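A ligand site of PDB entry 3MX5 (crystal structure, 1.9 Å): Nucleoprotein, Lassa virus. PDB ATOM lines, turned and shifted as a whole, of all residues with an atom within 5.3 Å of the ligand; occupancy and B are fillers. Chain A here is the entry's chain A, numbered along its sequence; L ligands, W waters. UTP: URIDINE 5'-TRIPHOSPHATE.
The guanidinium group (NH2) of Arg 331 sits at hydrogen-bond distance from the backbone carbonyl oxygen (O) of Thr 186 (2.6 Å).
The side-chain amino group (NZ) of Lys 261 sits at hydrogen-bond distance from the side-chain hydroxyl (OG1) of Thr 186.
NZ of Lys 261 is in hydrogen-bond range of O of Tyr 327 (3.0 Å).
NZ of Lys 317 sits at hydrogen-bond distance from OD1 of Asn 313, 2.8 Å away.
O of Leu 128 lies within hydrogen-bond range of N of Trp 172 (2.7 Å).
NH2 of Arg 308 lies within salt-bridge range of O1A of the ligand (2.7 Å).
O2B of the ligand is in salt-bridge range of NH1 of Arg 331 (2.8 Å).
The side-chain amino group (NZ) of Lys 261 lies within salt-bridge range of an oxygen (O2B) of the ligand (3.3 Å).
N of Asn 248 sits at hydrogen-bond distance from O2' of the ligand, at 3.0 Å.
An oxygen (O2B) of the ligand lies within salt-bridge range of the side-chain amino group of Lys 317, 3.6 Å away.
An oxygen (O1B) of the ligand is in hydrogen-bond range of the backbone NH (N) of Thr 186 (3.1 Å).
An oxygen (O1B) of the ligand is in hydrogen-bond range of the side-chain hydroxyl (OG1) of Thr 186 (3.2 Å).
Water W1 bridges the guanidinium group of Arg 308 (2.7 Å) and an oxygen (O1A) of the ligand (3.1 Å).
The backbone carbonyl oxygen (O) of Ile 249 sits close to an oxygen (O2) of the ligand, 3.1 Å away.
OE2 of Glu 125 touches C3' of the ligand, at 3.5 Å.
Leu 128 touches the ligand.
Trp 172 touches the ligand (CD1 to O4, 3.9 Å).
CB of Leu 180 touches O4 of the ligand, 3.4 Å away.
CD1 of Phe 184 touches O2 of the ligand (3.2 Å).
Gly 185 touches the ligand.
Ser 246 touches the ligand.
CA of Leu 247 touches O2' of the ligand (3.2 Å).
Within 4 Å of the ligand: Glu 125, Leu 128, Trp 172, Leu 180, Phe 184, Gly 185, Thr 186, Ser 246, Leu 247, Asn 248, Ile 249, Lys 261, Arg 308, Lys 317 and Arg 331.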
ATOM      1  N   MET A  62      -5.758 -31.646 -16.241  1.00  0.00           N
ATOM      2  CA  MET A  62      -5.640 -31.192 -14.831  1.00  0.00           C
ATOM      3  C   MET A  62      -6.819 -31.600 -13.944  1.00  0.00           C
ATOM      4  O   MET A  62      -6.711 -31.641 -12.707  1.00  0.00           O
ATOM      5  CB  MET A  62      -5.404 -29.674 -14.770  1.00  0.00           C
ATOM      6  CG  MET A  62      -4.029 -29.289 -15.371  1.00  0.00           C
ATOM      7  SD  MET A  62      -2.618 -29.880 -14.390  1.00  0.00           S
ATOM      8  CE  MET A  62      -2.623 -28.715 -13.032  1.00  0.00           C
ATOM      9  N   THR A 124       5.547 -28.735   0.346  1.00  0.00           N
ATOM     10  CA  THR A 124       4.269 -28.434  -0.299  1.00  0.00           C
ATOM     11  C   THR A 124       4.110 -29.160  -1.635  1.00  0.00           C
ATOM     12  O   THR A 124       3.067 -29.740  -1.920  1.00  0.00           O
ATOM     13  CB  THR A 124       4.088 -26.912  -0.544  1.00  0.00           C
ATOM     14  OG1 THR A 124       4.073 -26.232   0.719  1.00  0.00           O
ATOM     15  CG2 THR A 124       2.773 -26.631  -1.248  1.00  0.00           C
ATOM     16  N   GLU A 125       5.178 -29.153  -2.422  1.00  0.00           N
ATOM     17  CA  GLU A 125       5.101 -29.598  -3.807  1.00  0.00           C
ATOM     18  C   GLU A 125       5.580 -31.033  -4.029  1.00  0.00           C
ATOM     19  O   GLU A 125       5.009 -31.748  -4.840  1.00  0.00           O
ATOM     20  CB  GLU A 125       5.872 -28.643  -4.698  1.00  0.00           C
ATOM     21  CG  GLU A 125       5.368 -27.209  -4.651  1.00  0.00           C
ATOM     22  CD  GLU A 125       6.160 -26.333  -5.581  1.00  0.00           C
ATOM     23  OE1 GLU A 125       7.143 -26.837  -6.189  1.00  0.00           O
ATOM     24  OE2 GLU A 125       5.825 -25.151  -5.710  1.00  0.00           O
ATOM     25  N   LEU A 128       3.237 -34.232  -4.226  1.00  0.00           N
ATOM     26  CA  LEU A 128       2.493 -34.343  -5.488  1.00  0.00           C
ATOM     27  C   LEU A 128       3.090 -35.341  -6.473  1.00  0.00           C
ATOM     28  O   LEU A 128       2.388 -35.882  -7.320  1.00  0.00           O
ATOM     29  CB  LEU A 128       2.428 -32.984  -6.196  1.00  0.00           C
ATOM     30  CG  LEU A 128       1.589 -31.914  -5.533  1.00  0.00           C
ATOM     31  CD1 LEU A 128       2.022 -30.579  -6.101  1.00  0.00           C
ATOM     32  CD2 LEU A 128       0.114 -32.185  -5.758  1.00  0.00           C
ATOM     33  N   ILE A 152      -1.912 -29.286   1.299  1.00  0.00           N
ATOM     34  CA  ILE A 152      -1.156 -29.108   0.084  1.00  0.00           C
ATOM     35  C   ILE A 152      -1.978 -29.319  -1.183  1.00  0.00           C
ATOM     36  O   ILE A 152      -1.438 -29.308  -2.271  1.00  0.00           O
ATOM     37  CB  ILE A 152       0.125 -29.974   0.071  1.00  0.00           C
ATOM     38  CG1 ILE A 152      -0.216 -31.469   0.023  1.00  0.00           C
ATOM     39  CG2 ILE A 152       1.057 -29.606   1.272  1.00  0.00           C
ATOM     40  CD1 ILE A 152       1.021 -32.316  -0.301  1.00  0.00           C
ATOM     41  N   TRP A 172       1.367 -36.722  -9.689  1.00  0.00           N
ATOM     42  CA  TRP A 172       2.205 -36.891 -10.872  1.00  0.00           C
ATOM     43  C   TRP A 172       3.056 -38.150 -10.807  1.00  0.00           C
ATOM     44  O   TRP A 172       3.887 -38.297  -9.902  1.00  0.00           O
ATOM     45  CB  TRP A 172       3.094 -35.676 -11.102  1.00  0.00           C
ATOM     46  CG  TRP A 172       2.337 -34.434 -11.515  1.00  0.00           C
ATOM     47  CD1 TRP A 172       1.962 -33.403 -10.709  1.00  0.00           C
ATOM     48  CD2 TRP A 172       1.870 -34.112 -12.833  1.00  0.00           C
ATOM     49  NE1 TRP A 172       1.286 -32.445 -11.454  1.00  0.00           N
ATOM     50  CE2 TRP A 172       1.244 -32.851 -12.757  1.00  0.00           C
ATOM     51  CE3 TRP A 172       1.968 -34.750 -14.079  1.00  0.00           C
ATOM     52  CZ2 TRP A 172       0.672 -32.234 -13.875  1.00  0.00           C
ATOM     53  CZ3 TRP A 172       1.396 -34.134 -15.197  1.00  0.00           C
ATOM     54  CH2 TRP A 172       0.745 -32.881 -15.077  1.00  0.00           C
ATOM     55  N   LEU A 180       8.394 -30.730 -13.646  1.00  0.00           N
ATOM     56  CA  LEU A 180       7.261 -30.020 -13.078  1.00  0.00           C
ATOM     57  C   LEU A 180       7.685 -28.584 -12.747  1.00  0.00           C
ATOM     58  O   LEU A 180       6.839 -27.665 -12.734  1.00  0.00           O
ATOM     59  CB  LEU A 180       6.696 -30.758 -11.850  1.00  0.00           C
ATOM     60  CG  LEU A 180       6.348 -32.224 -12.105  1.00  0.00           C
ATOM     61  CD1 LEU A 180       6.331 -33.118 -10.831  1.00  0.00           C
ATOM     62  CD2 LEU A 180       5.011 -32.326 -12.849  1.00  0.00           C
ATOM     63  N   PHE A 184       3.436 -24.311 -13.624  1.00  0.00           N
ATOM     64  CA  PHE A 184       2.115 -24.139 -13.048  1.00  0.00           C
ATOM     65  C   PHE A 184       1.670 -22.682 -12.721  1.00  0.00           C
ATOM     66  O   PHE A 184       0.553 -22.434 -12.284  1.00  0.00           O
ATOM     67  CB  PHE A 184       1.993 -25.105 -11.856  1.00  0.00           C
ATOM     68  CG  PHE A 184       2.157 -26.541 -12.254  1.00  0.00           C
ATOM     69  CD1 PHE A 184       1.091 -27.265 -12.765  1.00  0.00           C
ATOM     70  CD2 PHE A 184       3.429 -27.160 -12.186  1.00  0.00           C
ATOM     71  CE1 PHE A 184       1.247 -28.623 -13.152  1.00  0.00           C
ATOM     72  CE2 PHE A 184       3.618 -28.508 -12.599  1.00  0.00           C
ATOM     73  CZ  PHE A 184       2.498 -29.240 -13.075  1.00  0.00           C
ATOM     74  N   GLY A 185       2.575 -21.733 -12.959  1.00  0.00           N
ATOM     75  CA  GLY A 185       2.348 -20.327 -12.662  1.00  0.00           C
ATOM     76  C   GLY A 185       1.261 -19.609 -13.454  1.00  0.00           C
ATOM     77  O   GLY A 185       1.039 -19.834 -14.651  1.00  0.00           O
ATOM     78  N   THR A 186       0.574 -18.707 -12.776  1.00  0.00           N
ATOM     79  CA  THR A 186      -0.489 -17.911 -13.450  1.00  0.00           C
ATOM     80  C   THR A 186       0.082 -16.655 -14.045  1.00  0.00           C
ATOM     81  O   THR A 186       1.015 -16.079 -13.478  1.00  0.00           O
ATOM     82  CB  THR A 186      -1.560 -17.451 -12.450  1.00  0.00           C
ATOM     83  OG1 THR A 186      -0.926 -16.779 -11.337  1.00  0.00           O
ATOM     84  CG2 THR A 186      -2.370 -18.628 -11.971  1.00  0.00           C
ATOM     85  N   SER A 246      -4.990 -22.103  -4.625  1.00  0.00           N
ATOM     86  CA  SER A 246      -3.745 -21.878  -5.381  1.00  0.00           C
ATOM     87  C   SER A 246      -2.978 -23.166  -5.706  1.00  0.00           C
ATOM     88  O   SER A 246      -2.165 -23.192  -6.630  1.00  0.00           O
ATOM     89  CB  SER A 246      -2.794 -20.893  -4.642  1.00  0.00           C
ATOM     90  OG  SER A 246      -1.454 -20.990  -5.164  1.00  0.00           O
ATOM     91  N   LEU A 247      -3.238 -24.230  -4.963  1.00  0.00           N
ATOM     92  CA  LEU A 247      -2.389 -25.426  -5.054  1.00  0.00           C
ATOM     93  C   LEU A 247      -2.870 -26.485  -6.056  1.00  0.00           C
ATOM     94  O   LEU A 247      -4.068 -26.592  -6.347  1.00  0.00           O
ATOM     95  CB  LEU A 247      -2.164 -26.033  -3.671  1.00  0.00           C
ATOM     96  CG  LEU A 247      -1.898 -25.008  -2.560  1.00  0.00           C
ATOM     97  CD1 LEU A 247      -2.492 -25.482  -1.231  1.00  0.00           C
ATOM     98  CD2 LEU A 247      -0.386 -24.661  -2.453  1.00  0.00           C
ATOM     99  N   ASN A 248      -1.915 -27.250  -6.575  1.00  0.00           N
ATOM    100  CA  ASN A 248      -2.177 -28.368  -7.508  1.00  0.00           C
ATOM    101  C   ASN A 248      -2.884 -28.005  -8.829  1.00  0.00           C
ATOM    102  O   ASN A 248      -3.393 -28.887  -9.540  1.00  0.00           O
ATOM    103  CB  ASN A 248      -2.920 -29.521  -6.819  1.00  0.00           C
ATOM    104  CG  ASN A 248      -2.843 -30.803  -7.624  1.00  0.00           C
ATOM    105  OD1 ASN A 248      -1.903 -30.991  -8.390  1.00  0.00           O
ATOM    106  ND2 ASN A 248      -3.842 -31.668  -7.468  1.00  0.00           N
ATOM    107  N   ILE A 249      -2.879 -26.721  -9.170  1.00  0.00           N
ATOM    108  CA  ILE A 249      -3.553 -26.285 -10.377  1.00  0.00           C
ATOM    109  C   ILE A 249      -2.569 -25.671 -11.349  1.00  0.00           C
ATOM    110  O   ILE A 249      -1.372 -25.874 -11.221  1.00  0.00           O
ATOM    111  CB  ILE A 249      -4.710 -25.291 -10.084  1.00  0.00           C
ATOM    112  CG1 ILE A 249      -4.266 -24.227  -9.088  1.00  0.00           C
ATOM    113  CG2 ILE A 249      -5.942 -26.054  -9.619  1.00  0.00           C
ATOM    114  CD1 ILE A 249      -4.701 -22.818  -9.466  1.00  0.00           C
ATOM    115  N   GLY A 257      -7.156 -16.228  -7.175  1.00  0.00           N
ATOM    116  CA  GLY A 257      -5.750 -15.788  -7.221  1.00  0.00           C
ATOM    117  C   GLY A 257      -5.286 -15.300  -8.580  1.00  0.00           C
ATOM    118  O   GLY A 257      -4.625 -14.239  -8.702  1.00  0.00           O
ATOM    119  N   ALA A 258      -5.643 -16.053  -9.629  1.00  0.00           N
ATOM    120  CA  ALA A 258      -5.362 -15.648 -11.001  1.00  0.00           C
ATOM    121  C   ALA A 258      -6.013 -14.321 -11.410  1.00  0.00           C
ATOM    122  O   ALA A 258      -5.360 -13.445 -12.014  1.00  0.00           O
ATOM    123  CB  ALA A 258      -5.783 -16.743 -11.984  1.00  0.00           C
ATOM    124  N   LYS A 261      -4.563 -11.144  -9.604  1.00  0.00           N
ATOM    125  CA  LYS A 261      -3.290 -10.746 -10.226  1.00  0.00           C
ATOM    126  C   LYS A 261      -3.470 -10.028 -11.579  1.00  0.00           C
ATOM    127  O   LYS A 261      -2.842  -8.984 -11.872  1.00  0.00           O
ATOM    128  CB  LYS A 261      -2.361 -11.988 -10.329  1.00  0.00           C
ATOM    129  CG  LYS A 261      -1.009 -11.723 -10.948  1.00  0.00           C
ATOM    130  CD  LYS A 261      -0.259 -13.039 -11.363  1.00  0.00           C
ATOM    131  CE  LYS A 261      -0.008 -13.982 -10.186  1.00  0.00           C
ATOM    132  NZ  LYS A 261       1.032 -15.035 -10.578  1.00  0.00           N
ATOM    133  N   ARG A 308       1.131 -19.526   0.405  1.00  0.00           N
ATOM    134  CA  ARG A 308       2.182 -18.596   0.837  1.00  0.00           C
ATOM    135  C   ARG A 308       1.648 -17.287   1.385  1.00  0.00           C
ATOM    136  O   ARG A 308       0.770 -16.661   0.778  1.00  0.00           O
ATOM    137  CB  ARG A 308       3.137 -18.278  -0.297  1.00  0.00           C
ATOM    138  CG  ARG A 308       3.939 -19.429  -0.775  1.00  0.00           C
ATOM    139  CD  ARG A 308       4.609 -18.999  -2.037  1.00  0.00           C
ATOM    140  NE  ARG A 308       4.956 -20.113  -2.904  1.00  0.00           N
ATOM    141  CZ  ARG A 308       5.422 -19.927  -4.132  1.00  0.00           C
ATOM    142  NH1 ARG A 308       5.605 -18.685  -4.583  1.00  0.00           N
ATOM    143  NH2 ARG A 308       5.715 -20.974  -4.900  1.00  0.00           N
ATOM    144  N   ASN A 313       5.833 -15.224  -0.505  1.00  0.00           N
ATOM    145  CA  ASN A 313       5.523 -15.037  -1.932  1.00  0.00           C
ATOM    146  C   ASN A 313       6.525 -14.131  -2.650  1.00  0.00           C
ATOM    147  O   ASN A 313       7.169 -14.547  -3.625  1.00  0.00           O
ATOM    148  CB  ASN A 313       4.090 -14.556  -2.086  1.00  0.00           C
ATOM    149  CG  ASN A 313       3.594 -14.605  -3.540  1.00  0.00           C
ATOM    150  OD1 ASN A 313       3.716 -15.627  -4.244  1.00  0.00           O
ATOM    151  ND2 ASN A 313       3.044 -13.491  -3.986  1.00  0.00           N
ATOM    152  N   LYS A 317       9.318 -15.381  -5.468  1.00  0.00           N
ATOM    153  CA  LYS A 317       9.257 -14.852  -6.823  1.00  0.00           C
ATOM    154  C   LYS A 317      10.510 -14.064  -7.244  1.00  0.00           C
ATOM    155  O   LYS A 317      11.017 -14.264  -8.363  1.00  0.00           O
ATOM    156  CB  LYS A 317       7.978 -14.025  -7.072  1.00  0.00           C
ATOM    157  CG  LYS A 317       6.710 -14.868  -7.345  1.00  0.00           C
ATOM    158  CD  LYS A 317       5.459 -13.987  -7.136  1.00  0.00           C
ATOM    159  CE  LYS A 317       4.206 -14.671  -7.730  1.00  0.00           C
ATOM    160  NZ  LYS A 317       3.831 -15.924  -7.004  1.00  0.00           N
ATOM    161  N   TYR A 327       6.207 -11.393 -10.718  1.00  0.00           N
ATOM    162  CA  TYR A 327       4.827 -11.723 -10.391  1.00  0.00           C
ATOM    163  C   TYR A 327       3.997 -12.190 -11.590  1.00  0.00           C
ATOM    164  O   TYR A 327       3.138 -13.015 -11.400  1.00  0.00           O
ATOM    165  CB  TYR A 327       4.077 -10.583  -9.684  1.00  0.00           C
ATOM    166  CG  TYR A 327       4.281 -10.470  -8.211  1.00  0.00           C
ATOM    167  CD1 TYR A 327       3.388 -11.064  -7.291  1.00  0.00           C
ATOM    168  CD2 TYR A 327       5.359  -9.766  -7.705  1.00  0.00           C
ATOM    169  CE1 TYR A 327       3.589 -10.944  -5.927  1.00  0.00           C
ATOM    170  CE2 TYR A 327       5.568  -9.651  -6.344  1.00  0.00           C
ATOM    171  CZ  TYR A 327       4.683 -10.225  -5.462  1.00  0.00           C
ATOM    172  OH  TYR A 327       4.955 -10.070  -4.131  1.00  0.00           O
ATOM    173  N   ARG A 331       7.141 -17.668 -16.804  1.00  0.00           N
ATOM    174  CA  ARG A 331       8.220 -18.200 -15.984  1.00  0.00           C
ATOM    175  C   ARG A 331       8.476 -19.677 -16.400  1.00  0.00           C
ATOM    176  O   ARG A 331       9.368 -20.374 -15.862  1.00  0.00           O
ATOM    177  CB  ARG A 331       7.811 -18.090 -14.499  1.00  0.00           C
ATOM    178  CG  ARG A 331       8.186 -16.748 -13.845  1.00  0.00           C
ATOM    179  CD  ARG A 331       7.189 -16.274 -12.780  1.00  0.00           C
ATOM    180  NE  ARG A 331       5.907 -15.990 -13.411  1.00  0.00           N
ATOM    181  CZ  ARG A 331       4.727 -16.423 -12.994  1.00  0.00           C
ATOM    182  NH1 ARG A 331       4.617 -17.125 -11.873  1.00  0.00           N
ATOM    183  NH2 ARG A 331       3.637 -16.113 -13.713  1.00  0.00           N
HETATM  184  PA  UTP L   1       3.245 -20.323  -8.084  1.00  0.00           P
HETATM  185  O1A UTP L   1       4.447 -20.379  -7.240  1.00  0.00           O
HETATM  186  O2A UTP L   1       3.678 -20.430  -9.635  1.00  0.00           O
HETATM  187  O3A UTP L   1       2.510 -18.935  -7.713  1.00  0.00           O
HETATM  188  O5' UTP L   1       2.238 -21.526  -7.736  1.00  0.00           O
HETATM  189  PB  UTP L   1       1.778 -18.156  -8.919  1.00  0.00           P
HETATM  190  O1B UTP L   1       0.654 -18.972  -9.663  1.00  0.00           O
HETATM  191  O2B UTP L   1       2.765 -17.751  -9.928  1.00  0.00           O
HETATM  192  O3B UTP L   1       1.185 -16.783  -8.248  1.00  0.00           O
HETATM  193  PG  UTP L   1      -0.015 -17.098  -7.190  1.00  0.00           P
HETATM  194  O1G UTP L   1       0.457 -18.136  -6.065  1.00  0.00           O
HETATM  195  O2G UTP L   1      -1.197 -17.593  -7.933  1.00  0.00           O
HETATM  196  O3G UTP L   1      -0.441 -15.755  -6.440  1.00  0.00           O
HETATM  197  C5' UTP L   1       2.997 -22.730  -7.731  1.00  0.00           C
HETATM  198  C4' UTP L   1       2.030 -23.866  -7.359  1.00  0.00           C
HETATM  199  O4' UTP L   1       2.139 -24.914  -8.352  1.00  0.00           O
HETATM  200  C1' UTP L   1       1.559 -26.085  -7.757  1.00  0.00           C
HETATM  201  C2' UTP L   1       1.872 -26.006  -6.245  1.00  0.00           C
HETATM  202  O2' UTP L   1       0.697 -26.329  -5.505  1.00  0.00           O
HETATM  203  C3' UTP L   1       2.383 -24.562  -6.018  1.00  0.00           C
HETATM  204  O3' UTP L   1       1.719 -23.948  -4.911  1.00  0.00           O
HETATM  205  N1  UTP L   1       2.254 -27.269  -8.262  1.00  0.00           N
HETATM  206  C6  UTP L   1       3.490 -27.570  -7.742  1.00  0.00           C
HETATM  207  C2  UTP L   1       1.696 -28.042  -9.220  1.00  0.00           C
HETATM  208  O2  UTP L   1       0.606 -27.752  -9.674  1.00  0.00           O
HETATM  209  N3  UTP L   1       2.362 -29.136  -9.661  1.00  0.00           N
HETATM  210  C4  UTP L   1       3.585 -29.469  -9.154  1.00  0.00           C
HETATM  211  O4  UTP L   1       4.200 -30.440  -9.544  1.00  0.00           O
HETATM  212  C5  UTP L   1       4.173 -28.654  -8.158  1.00  0.00           C
HETATM  213  O   HOH W   1       7.347 -21.324  -7.057  1.00  0.00           O
